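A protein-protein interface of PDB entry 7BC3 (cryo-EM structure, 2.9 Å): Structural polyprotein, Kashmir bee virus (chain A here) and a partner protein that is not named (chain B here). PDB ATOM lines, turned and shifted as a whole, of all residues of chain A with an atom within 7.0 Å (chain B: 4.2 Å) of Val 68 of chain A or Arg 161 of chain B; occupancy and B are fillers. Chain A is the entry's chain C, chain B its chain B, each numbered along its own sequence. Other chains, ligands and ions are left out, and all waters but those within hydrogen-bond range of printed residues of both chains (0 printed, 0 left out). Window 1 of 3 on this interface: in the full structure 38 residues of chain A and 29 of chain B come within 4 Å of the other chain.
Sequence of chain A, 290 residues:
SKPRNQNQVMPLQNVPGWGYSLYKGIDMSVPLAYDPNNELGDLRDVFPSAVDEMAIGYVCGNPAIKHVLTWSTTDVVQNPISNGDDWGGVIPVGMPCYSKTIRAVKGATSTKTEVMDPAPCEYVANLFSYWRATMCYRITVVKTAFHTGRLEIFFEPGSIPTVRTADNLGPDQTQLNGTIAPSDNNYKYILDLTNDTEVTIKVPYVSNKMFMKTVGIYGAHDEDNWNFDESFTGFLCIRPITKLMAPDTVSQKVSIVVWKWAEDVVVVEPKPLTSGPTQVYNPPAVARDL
OD2 of Asp 85 of chain A is in salt-bridge range of NH2 of Arg 161 of chain B (2.8 Å).
N of Ile 65 of chain A lies within hydrogen-bond range of OG1 of Thr 165 of chain B (2.9 Å).
The side-chain carboxylate (OD2) of Asp 85 of chain A lies within salt-bridge range of the guanidinium group (NH1) of Arg 82 of chain B (2.8 Å).
The side-chain carboxylate (OD1) of Asp 117 of chain A lies within salt-bridge range of the guanidinium group (NE) of Arg 82 of chain B (2.5 Å).
The guanidinium group of Arg 82 of chain B lies within hydrogen-bond range of the backbone carbonyl oxygen of Lys 66 of chain A (3.1 Å).
The guanidinium group of Arg 161 of chain B is in hydrogen-bond range of the backbone carbonyl oxygen of Lys 66 of chain A.
Val 68 of chain A touches just one residue of chain B: Arg 161.
Arg 161 of chain B touches five residues of chain A.
Printed residues of chain B within 4 Å of Ile 65 of chain A: Arg 161, Ala 162 and Thr 165.
Of the printed residues of chain A, Ala 162 of chain B touches Ala 64, Ile 65, Asp 117 and Pro 118.
Gly 163 of chain B touches none of the printed residues of chain A.
Val 258 of chain A touches none of the printed residues of chain B.
The nearest printed residue of chain B that does not touch Val 68 of chain A is Arg 82 of chain B (6.1 Å).
The backbone carbonyl oxygen (O) of Val 258 of chain A lies within hydrogen-bond range of the backbone NH (N) of Lys 66 of chain A, 3.1 Å away.
N of Gly 163 of chain B is in hydrogen-bond range of OG of Ser 160 of chain B, at 3.3 Å.
NZ of Lys 66 of chain A lies within salt-bridge range of OD1 of Asp 117 of chain A, at 3.1 Å.
The backbone carbonyl oxygen of Ala 162 of chain B sits at hydrogen-bond distance from the side-chain hydroxyl of Thr 165 of chain B (2.9 Å).
The backbone carbonyl oxygen (O) of His 67 of chain A is in hydrogen-bond range of the backbone NH (N) of Val 258 of chain A (3.0 Å).
The backbone carbonyl oxygen of Arg 161 of chain B sits at hydrogen-bond distance from the side-chain hydroxyl of Thr 165 of chain B.
Of the 18 printed residues of chain A, 8 touch a printed residue of chain B.
Hydrophobic or aromatic side chains of chain A within 4 Å of the printed part of chain B: Ala 64, Ile 65 and Val 68.
Along chain A the printed residues that touch a printed residue of chain B span positions 64 to 118.
Hydrophobic or aromatic side chains of chain B that line the printed part of chain A: Ala 162.
Ala 162 of chain B touches Ala 64 of chain A.
Ala 64 of chain A touches Thr 165 of chain B (CA to OG1, 3.5 Å).
Arg 161 of chain B touches Ile 65 of chain A (NE to CG2, 3.5 Å).
Ala 162 of chain B touches Ile 65 of chain A.
N of His 67 of chain A touches NH2 of Arg 161 of chain B, at 3.96 Å.
Val 68 of chain A touches Arg 161 of chain B (CG2 to NH1, 3.5 Å).
Ser 160 of chain B touches Asp 117 of chain A (OG to CA, 3.97 Å).
CB of Ala 162 of chain B touches O of Asp 117 of chain A, at 3.95 Å.
O of Pro 118 of chain A touches CB of Ala 162 of chain B, 3.8 Å away.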
ATOM      1  N   ALA A  64       6.396  28.878 -21.428  1.00  0.00           N
ATOM      2  CA  ALA A  64       6.459  27.430 -21.342  1.00  0.00           C
ATOM      3  C   ALA A  64       6.217  27.018 -19.900  1.00  0.00           C
ATOM      4  O   ALA A  64       6.521  27.764 -18.966  1.00  0.00           O
ATOM      5  CB  ALA A  64       7.807  26.895 -21.830  1.00  0.00           C
ATOM      6  N   ILE A  65       5.665  25.824 -19.730  1.00  0.00           N
ATOM      7  CA  ILE A  65       5.351  25.313 -18.402  1.00  0.00           C
ATOM      8  C   ILE A  65       6.621  24.777 -17.759  1.00  0.00           C
ATOM      9  O   ILE A  65       7.334  23.955 -18.347  1.00  0.00           O
ATOM     10  CB  ILE A  65       4.266  24.229 -18.480  1.00  0.00           C
ATOM     11  CG1 ILE A  65       2.890  24.877 -18.595  1.00  0.00           C
ATOM     12  CG2 ILE A  65       4.316  23.327 -17.261  1.00  0.00           C
ATOM     13  CD1 ILE A  65       1.825  23.948 -19.097  1.00  0.00           C
ATOM     14  N   LYS A  66       6.902  25.244 -16.543  1.00  0.00           N
ATOM     15  CA  LYS A  66       8.059  24.806 -15.782  1.00  0.00           C
ATOM     16  C   LYS A  66       7.702  24.112 -14.479  1.00  0.00           C
ATOM     17  O   LYS A  66       8.531  23.360 -13.957  1.00  0.00           O
ATOM     18  CB  LYS A  66       8.969  25.998 -15.459  1.00  0.00           C
ATOM     19  CG  LYS A  66       9.583  26.658 -16.678  1.00  0.00           C
ATOM     20  CD  LYS A  66      10.652  25.793 -17.314  1.00  0.00           C
ATOM     21  CE  LYS A  66      11.860  25.648 -16.415  1.00  0.00           C
ATOM     22  NZ  LYS A  66      13.029  25.106 -17.145  1.00  0.00           N
ATOM     23  N   HIS A  67       6.505  24.339 -13.944  1.00  0.00           N
ATOM     24  CA  HIS A  67       6.077  23.737 -12.692  1.00  0.00           C
ATOM     25  C   HIS A  67       4.654  23.231 -12.846  1.00  0.00           C
ATOM     26  O   HIS A  67       3.789  23.949 -13.353  1.00  0.00           O
ATOM     27  CB  HIS A  67       6.138  24.743 -11.539  1.00  0.00           C
ATOM     28  CG  HIS A  67       7.520  25.211 -11.208  1.00  0.00           C
ATOM     29  ND1 HIS A  67       8.337  24.544 -10.321  1.00  0.00           N
ATOM     30  CD2 HIS A  67       8.223  26.286 -11.633  1.00  0.00           C
ATOM     31  CE1 HIS A  67       9.487  25.185 -10.218  1.00  0.00           C
ATOM     32  NE2 HIS A  67       9.445  26.245 -11.004  1.00  0.00           N
ATOM     33  N   VAL A  68       4.418  21.997 -12.409  1.00  0.00           N
ATOM     34  CA  VAL A  68       3.070  21.457 -12.247  1.00  0.00           C
ATOM     35  C   VAL A  68       3.051  20.798 -10.870  1.00  0.00           C
ATOM     36  O   VAL A  68       3.474  19.651 -10.704  1.00  0.00           O
ATOM     37  CB  VAL A  68       2.683  20.463 -13.344  1.00  0.00           C
ATOM     38  CG1 VAL A  68       1.222  20.075 -13.202  1.00  0.00           C
ATOM     39  CG2 VAL A  68       2.946  21.056 -14.715  1.00  0.00           C
ATOM     40  N   LEU A  69       2.561  21.525  -9.876  1.00  0.00           N
ATOM     41  CA  LEU A  69       2.552  21.071  -8.497  1.00  0.00           C
ATOM     42  C   LEU A  69       1.198  20.479  -8.139  1.00  0.00           C
ATOM     43  O   LEU A  69       0.193  20.717  -8.808  1.00  0.00           O
ATOM     44  CB  LEU A  69       2.882  22.223  -7.551  1.00  0.00           C
ATOM     45  CG  LEU A  69       4.296  22.782  -7.679  1.00  0.00           C
ATOM     46  CD1 LEU A  69       4.441  24.013  -6.814  1.00  0.00           C
ATOM     47  CD2 LEU A  69       5.325  21.734  -7.305  1.00  0.00           C
ATOM     48  N   THR A  70       1.189  19.699  -7.063  1.00  0.00           N
ATOM     49  CA  THR A  70      -0.013  19.041  -6.566  1.00  0.00           C
ATOM     50  C   THR A  70      -0.285  19.559  -5.162  1.00  0.00           C
ATOM     51  O   THR A  70       0.466  19.257  -4.228  1.00  0.00           O
ATOM     52  CB  THR A  70       0.149  17.523  -6.573  1.00  0.00           C
ATOM     53  OG1 THR A  70       0.429  17.077  -7.905  1.00  0.00           O
ATOM     54  CG2 THR A  70      -1.114  16.848  -6.076  1.00  0.00           C
ATOM     55  N   ASN A  83       4.881  18.871  -3.755  1.00  0.00           N
ATOM     56  CA  ASN A  83       4.419  17.585  -4.258  1.00  0.00           C
ATOM     57  C   ASN A  83       4.109  17.687  -5.744  1.00  0.00           C
ATOM     58  O   ASN A  83       3.390  18.595  -6.175  1.00  0.00           O
ATOM     59  CB  ASN A  83       3.180  17.123  -3.493  1.00  0.00           C
ATOM     60  CG  ASN A  83       3.468  16.852  -2.032  1.00  0.00           C
ATOM     61  OD1 ASN A  83       4.490  16.258  -1.689  1.00  0.00           O
ATOM     62  ND2 ASN A  83       2.570  17.292  -1.162  1.00  0.00           N
ATOM     63  N   GLY A  84       4.657  16.756  -6.521  1.00  0.00           N
ATOM     64  CA  GLY A  84       4.322  16.645  -7.926  1.00  0.00           C
ATOM     65  C   GLY A  84       5.485  16.885  -8.865  1.00  0.00           C
ATOM     66  O   GLY A  84       5.620  16.191  -9.877  1.00  0.00           O
ATOM     67  N   ASP A  85       6.330  17.864  -8.552  1.00  0.00           N
ATOM     68  CA  ASP A  85       7.417  18.249  -9.437  1.00  0.00           C
ATOM     69  C   ASP A  85       8.654  18.579  -8.615  1.00  0.00           C
ATOM     70  O   ASP A  85       8.587  18.754  -7.397  1.00  0.00           O
ATOM     71  CB  ASP A  85       7.027  19.455 -10.306  1.00  0.00           C
ATOM     72  CG  ASP A  85       7.831  19.541 -11.588  1.00  0.00           C
ATOM     73  OD1 ASP A  85       8.501  18.550 -11.945  1.00  0.00           O
ATOM     74  OD2 ASP A  85       7.793  20.604 -12.242  1.00  0.00           O
ATOM     75  N   ASP A  86       9.790  18.667  -9.301  1.00  0.00           N
ATOM     76  CA  ASP A  86      11.024  19.069  -8.650  1.00  0.00           C
ATOM     77  C   ASP A  86      11.006  20.573  -8.400  1.00  0.00           C
ATOM     78  O   ASP A  86      10.203  21.315  -8.970  1.00  0.00           O
ATOM     79  CB  ASP A  86      12.239  18.699  -9.505  1.00  0.00           C
ATOM     80  CG  ASP A  86      12.482  17.201  -9.569  1.00  0.00           C
ATOM     81  OD1 ASP A  86      13.276  16.762 -10.429  1.00  0.00           O
ATOM     82  OD2 ASP A  86      11.870  16.462  -8.772  1.00  0.00           O
ATOM     83  N   ASP A 117      15.733  21.168 -19.045  1.00  0.00           N
ATOM     84  CA  ASP A 117      14.380  21.311 -19.573  1.00  0.00           C
ATOM     85  C   ASP A 117      14.118  22.801 -19.750  1.00  0.00           C
ATOM     86  O   ASP A 117      13.435  23.426 -18.925  1.00  0.00           O
ATOM     87  CB  ASP A 117      13.360  20.672 -18.635  1.00  0.00           C
ATOM     88  CG  ASP A 117      13.448  21.223 -17.227  1.00  0.00           C
ATOM     89  OD1 ASP A 117      12.569  22.025 -16.849  1.00  0.00           O
ATOM     90  OD2 ASP A 117      14.399  20.868 -16.501  1.00  0.00           O
ATOM     91  N   PRO A 118      14.639  23.406 -20.816  1.00  0.00           N
ATOM     92  CA  PRO A 118      14.597  24.865 -20.920  1.00  0.00           C
ATOM     93  C   PRO A 118      13.385  25.399 -21.660  1.00  0.00           C
ATOM     94  O   PRO A 118      12.894  24.814 -22.628  1.00  0.00           O
ATOM     95  CB  PRO A 118      15.884  25.187 -21.690  1.00  0.00           C
ATOM     96  CG  PRO A 118      16.224  23.932 -22.448  1.00  0.00           C
ATOM     97  CD  PRO A 118      15.338  22.811 -21.964  1.00  0.00           C
ATOM     98  N   VAL A 142      -5.566  24.446 -11.495  1.00  0.00           N
ATOM     99  CA  VAL A 142      -6.515  23.549 -12.141  1.00  0.00           C
ATOM    100  C   VAL A 142      -7.430  23.013 -11.046  1.00  0.00           C
ATOM    101  O   VAL A 142      -7.030  22.176 -10.237  1.00  0.00           O
ATOM    102  CB  VAL A 142      -5.806  22.421 -12.891  1.00  0.00           C
ATOM    103  CG1 VAL A 142      -6.817  21.459 -13.463  1.00  0.00           C
ATOM    104  CG2 VAL A 142      -4.923  22.989 -13.988  1.00  0.00           C
ATOM    105  N   SER A 255      -3.927  20.948  -9.278  1.00  0.00           N
ATOM    106  CA  SER A 255      -2.641  21.093  -9.942  1.00  0.00           C
ATOM    107  C   SER A 255      -2.367  22.569 -10.179  1.00  0.00           C
ATOM    108  O   SER A 255      -3.235  23.295 -10.675  1.00  0.00           O
ATOM    109  CB  SER A 255      -2.609  20.325 -11.264  1.00  0.00           C
ATOM    110  OG  SER A 255      -2.631  18.928 -11.037  1.00  0.00           O
ATOM    111  N   ILE A 256      -1.168  23.009  -9.815  1.00  0.00           N
ATOM    112  CA  ILE A 256      -0.754  24.397  -9.962  1.00  0.00           C
ATOM    113  C   ILE A 256       0.221  24.457 -11.125  1.00  0.00           C
ATOM    114  O   ILE A 256       1.347  23.953 -11.033  1.00  0.00           O
ATOM    115  CB  ILE A 256      -0.120  24.949  -8.680  1.00  0.00           C
ATOM    116  CG1 ILE A 256      -1.124  24.903  -7.529  1.00  0.00           C
ATOM    117  CG2 ILE A 256       0.362  26.367  -8.899  1.00  0.00           C
ATOM    118  CD1 ILE A 256      -0.481  24.903  -6.178  1.00  0.00           C
ATOM    119  N   VAL A 257      -0.209  25.074 -12.219  1.00  0.00           N
ATOM    120  CA  VAL A 257       0.578  25.175 -13.438  1.00  0.00           C
ATOM    121  C   VAL A 257       1.195  26.563 -13.494  1.00  0.00           C
ATOM    122  O   VAL A 257       0.523  27.562 -13.209  1.00  0.00           O
ATOM    123  CB  VAL A 257      -0.291  24.899 -14.676  1.00  0.00           C
ATOM    124  CG1 VAL A 257       0.500  25.105 -15.949  1.00  0.00           C
ATOM    125  CG2 VAL A 257      -0.870  23.499 -14.606  1.00  0.00           C
ATOM    126  N   VAL A 258       2.473  26.628 -13.857  1.00  0.00           N
ATOM    127  CA  VAL A 258       3.234  27.870 -13.857  1.00  0.00           C
ATOM    128  C   VAL A 258       3.895  28.026 -15.217  1.00  0.00           C
ATOM    129  O   VAL A 258       4.730  27.201 -15.604  1.00  0.00           O
ATOM    130  CB  VAL A 258       4.292  27.900 -12.743  1.00  0.00           C
ATOM    131  CG1 VAL A 258       4.948  29.263 -12.669  1.00  0.00           C
ATOM    132  CG2 VAL A 258       3.677  27.530 -11.405  1.00  0.00           C
ATOM    133  N   LEU B  80       1.989  14.917 -19.098  1.00  0.00           N
ATOM    134  CA  LEU B  80       3.210  15.297 -19.795  1.00  0.00           C
ATOM    135  C   LEU B  80       4.397  15.245 -18.841  1.00  0.00           C
ATOM    136  O   LEU B  80       4.333  15.757 -17.720  1.00  0.00           O
ATOM    137  CB  LEU B  80       3.043  16.700 -20.378  1.00  0.00           C
ATOM    138  CG  LEU B  80       3.723  17.073 -21.692  1.00  0.00           C
ATOM    139  CD1 LEU B  80       3.467  16.052 -22.775  1.00  0.00           C
ATOM    140  CD2 LEU B  80       3.219  18.431 -22.134  1.00  0.00           C
ATOM    141  N   SER B  81       5.483  14.624 -19.290  1.00  0.00           N
ATOM    142  CA  SER B  81       6.637  14.373 -18.440  1.00  0.00           C
ATOM    143  C   SER B  81       7.617  15.538 -18.483  1.00  0.00           C
ATOM    144  O   SER B  81       7.729  16.248 -19.485  1.00  0.00           O
ATOM    145  CB  SER B  81       7.351  13.091 -18.863  1.00  0.00           C
ATOM    146  OG  SER B  81       8.287  12.686 -17.880  1.00  0.00           O
ATOM    147  N   ARG B  82       8.341  15.713 -17.378  1.00  0.00           N
ATOM    148  CA  ARG B  82       9.284  16.821 -17.270  1.00  0.00           C
ATOM    149  C   ARG B  82      10.480  16.619 -18.190  1.00  0.00           C
ATOM    150  O   ARG B  82      10.922  17.556 -18.863  1.00  0.00           O
ATOM    151  CB  ARG B  82       9.737  16.973 -15.818  1.00  0.00           C
ATOM    152  CG  ARG B  82      10.719  18.106 -15.579  1.00  0.00           C
ATOM    153  CD  ARG B  82      10.087  19.436 -15.898  1.00  0.00           C
ATOM    154  NE  ARG B  82      10.972  20.566 -15.642  1.00  0.00           N
ATOM    155  CZ  ARG B  82      11.064  21.201 -14.478  1.00  0.00           C
ATOM    156  NH1 ARG B  82      10.329  20.826 -13.442  1.00  0.00           N
ATOM    157  NH2 ARG B  82      11.899  22.222 -14.351  1.00  0.00           N
ATOM    158  N   GLN B  91       7.104  11.328 -24.810  1.00  0.00           N
ATOM    159  CA  GLN B  91       5.891  11.979 -24.347  1.00  0.00           C
ATOM    160  C   GLN B  91       4.675  11.261 -24.911  1.00  0.00           C
ATOM    161  O   GLN B  91       4.590  11.007 -26.115  1.00  0.00           O
ATOM    162  CB  GLN B  91       5.880  13.446 -24.767  1.00  0.00           C
ATOM    163  CG  GLN B  91       6.953  14.286 -24.109  1.00  0.00           C
ATOM    164  CD  GLN B  91       6.729  14.466 -22.624  1.00  0.00           C
ATOM    165  OE1 GLN B  91       5.825  13.868 -22.043  1.00  0.00           O
ATOM    166  NE2 GLN B  91       7.553  15.293 -22.002  1.00  0.00           N
ATOM    167  N   SER B 160      10.958  18.011 -23.894  1.00  0.00           N
ATOM    168  CA  SER B 160      10.467  18.173 -22.536  1.00  0.00           C
ATOM    169  C   SER B 160       9.100  18.848 -22.509  1.00  0.00           C
ATOM    170  O   SER B 160       8.620  19.400 -23.500  1.00  0.00           O
ATOM    171  CB  SER B 160      11.463  18.984 -21.711  1.00  0.00           C
ATOM    172  OG  SER B 160      11.767  20.212 -22.347  1.00  0.00           O
ATOM    173  N   ARG B 161       8.473  18.786 -21.332  1.00  0.00           N
ATOM    174  CA  ARG B 161       7.219  19.494 -21.106  1.00  0.00           C
ATOM    175  C   ARG B 161       7.346  20.965 -21.470  1.00  0.00           C
ATOM    176  O   ARG B 161       6.449  21.540 -22.097  1.00  0.00           O
ATOM    177  CB  ARG B 161       6.810  19.340 -19.643  1.00  0.00           C
ATOM    178  CG  ARG B 161       5.454  19.893 -19.297  1.00  0.00           C
ATOM    179  CD  ARG B 161       5.123  19.599 -17.855  1.00  0.00           C
ATOM    180  NE  ARG B 161       6.041  20.266 -16.939  1.00  0.00           N
ATOM    181  CZ  ARG B 161       6.264  19.874 -15.690  1.00  0.00           C
ATOM    182  NH1 ARG B 161       5.645  18.812 -15.198  1.00  0.00           N
ATOM    183  NH2 ARG B 161       7.112  20.547 -14.930  1.00  0.00           N
ATOM    184  N   ALA B 162       8.456  21.592 -21.082  1.00  0.00           N
ATOM    185  CA  ALA B 162       8.659  22.998 -21.409  1.00  0.00           C
ATOM    186  C   ALA B 162       8.765  23.198 -22.914  1.00  0.00           C
ATOM    187  O   ALA B 162       8.176  24.134 -23.466  1.00  0.00           O
ATOM    188  CB  ALA B 162       9.908  23.520 -20.709  1.00  0.00           C
ATOM    189  N   GLY B 163       9.508  22.327 -23.595  1.00  0.00           N
ATOM    190  CA  GLY B 163       9.575  22.417 -25.042  1.00  0.00           C
ATOM    191  C   GLY B 163       8.221  22.212 -25.688  1.00  0.00           C
ATOM    192  O   GLY B 163       7.791  23.006 -26.526  1.00  0.00           O
ATOM    193  N   VAL B 164       7.525  21.145 -25.295  1.00  0.00           N
ATOM    194  CA  VAL B 164       6.189  20.883 -25.829  1.00  0.00           C
ATOM    195  C   VAL B 164       5.315  22.121 -25.691  1.00  0.00           C
ATOM    196  O   VAL B 164       4.727  22.602 -26.666  1.00  0.00           O
ATOM    197  CB  VAL B 164       5.559  19.671 -25.121  1.00  0.00           C
ATOM    198  CG1 VAL B 164       4.153  19.443 -25.624  1.00  0.00           C
ATOM    199  CG2 VAL B 164       6.408  18.431 -25.329  1.00  0.00           C
ATOM    200  N   THR B 165       5.217  22.655 -24.475  1.00  0.00           N
ATOM    201  CA  THR B 165       4.423  23.853 -24.246  1.00  0.00           C
ATOM    202  C   THR B 165       4.998  25.078 -24.940  1.00  0.00           C
ATOM    203  O   THR B 165       4.311  26.100 -25.026  1.00  0.00           O
ATOM    204  CB  THR B 165       4.299  24.115 -22.750  1.00  0.00           C
ATOM    205  OG1 THR B 165       5.601  24.163 -22.157  1.00  0.00           O
ATOM    206  CG2 THR B 165       3.493  23.013 -22.098  1.00  0.00           C
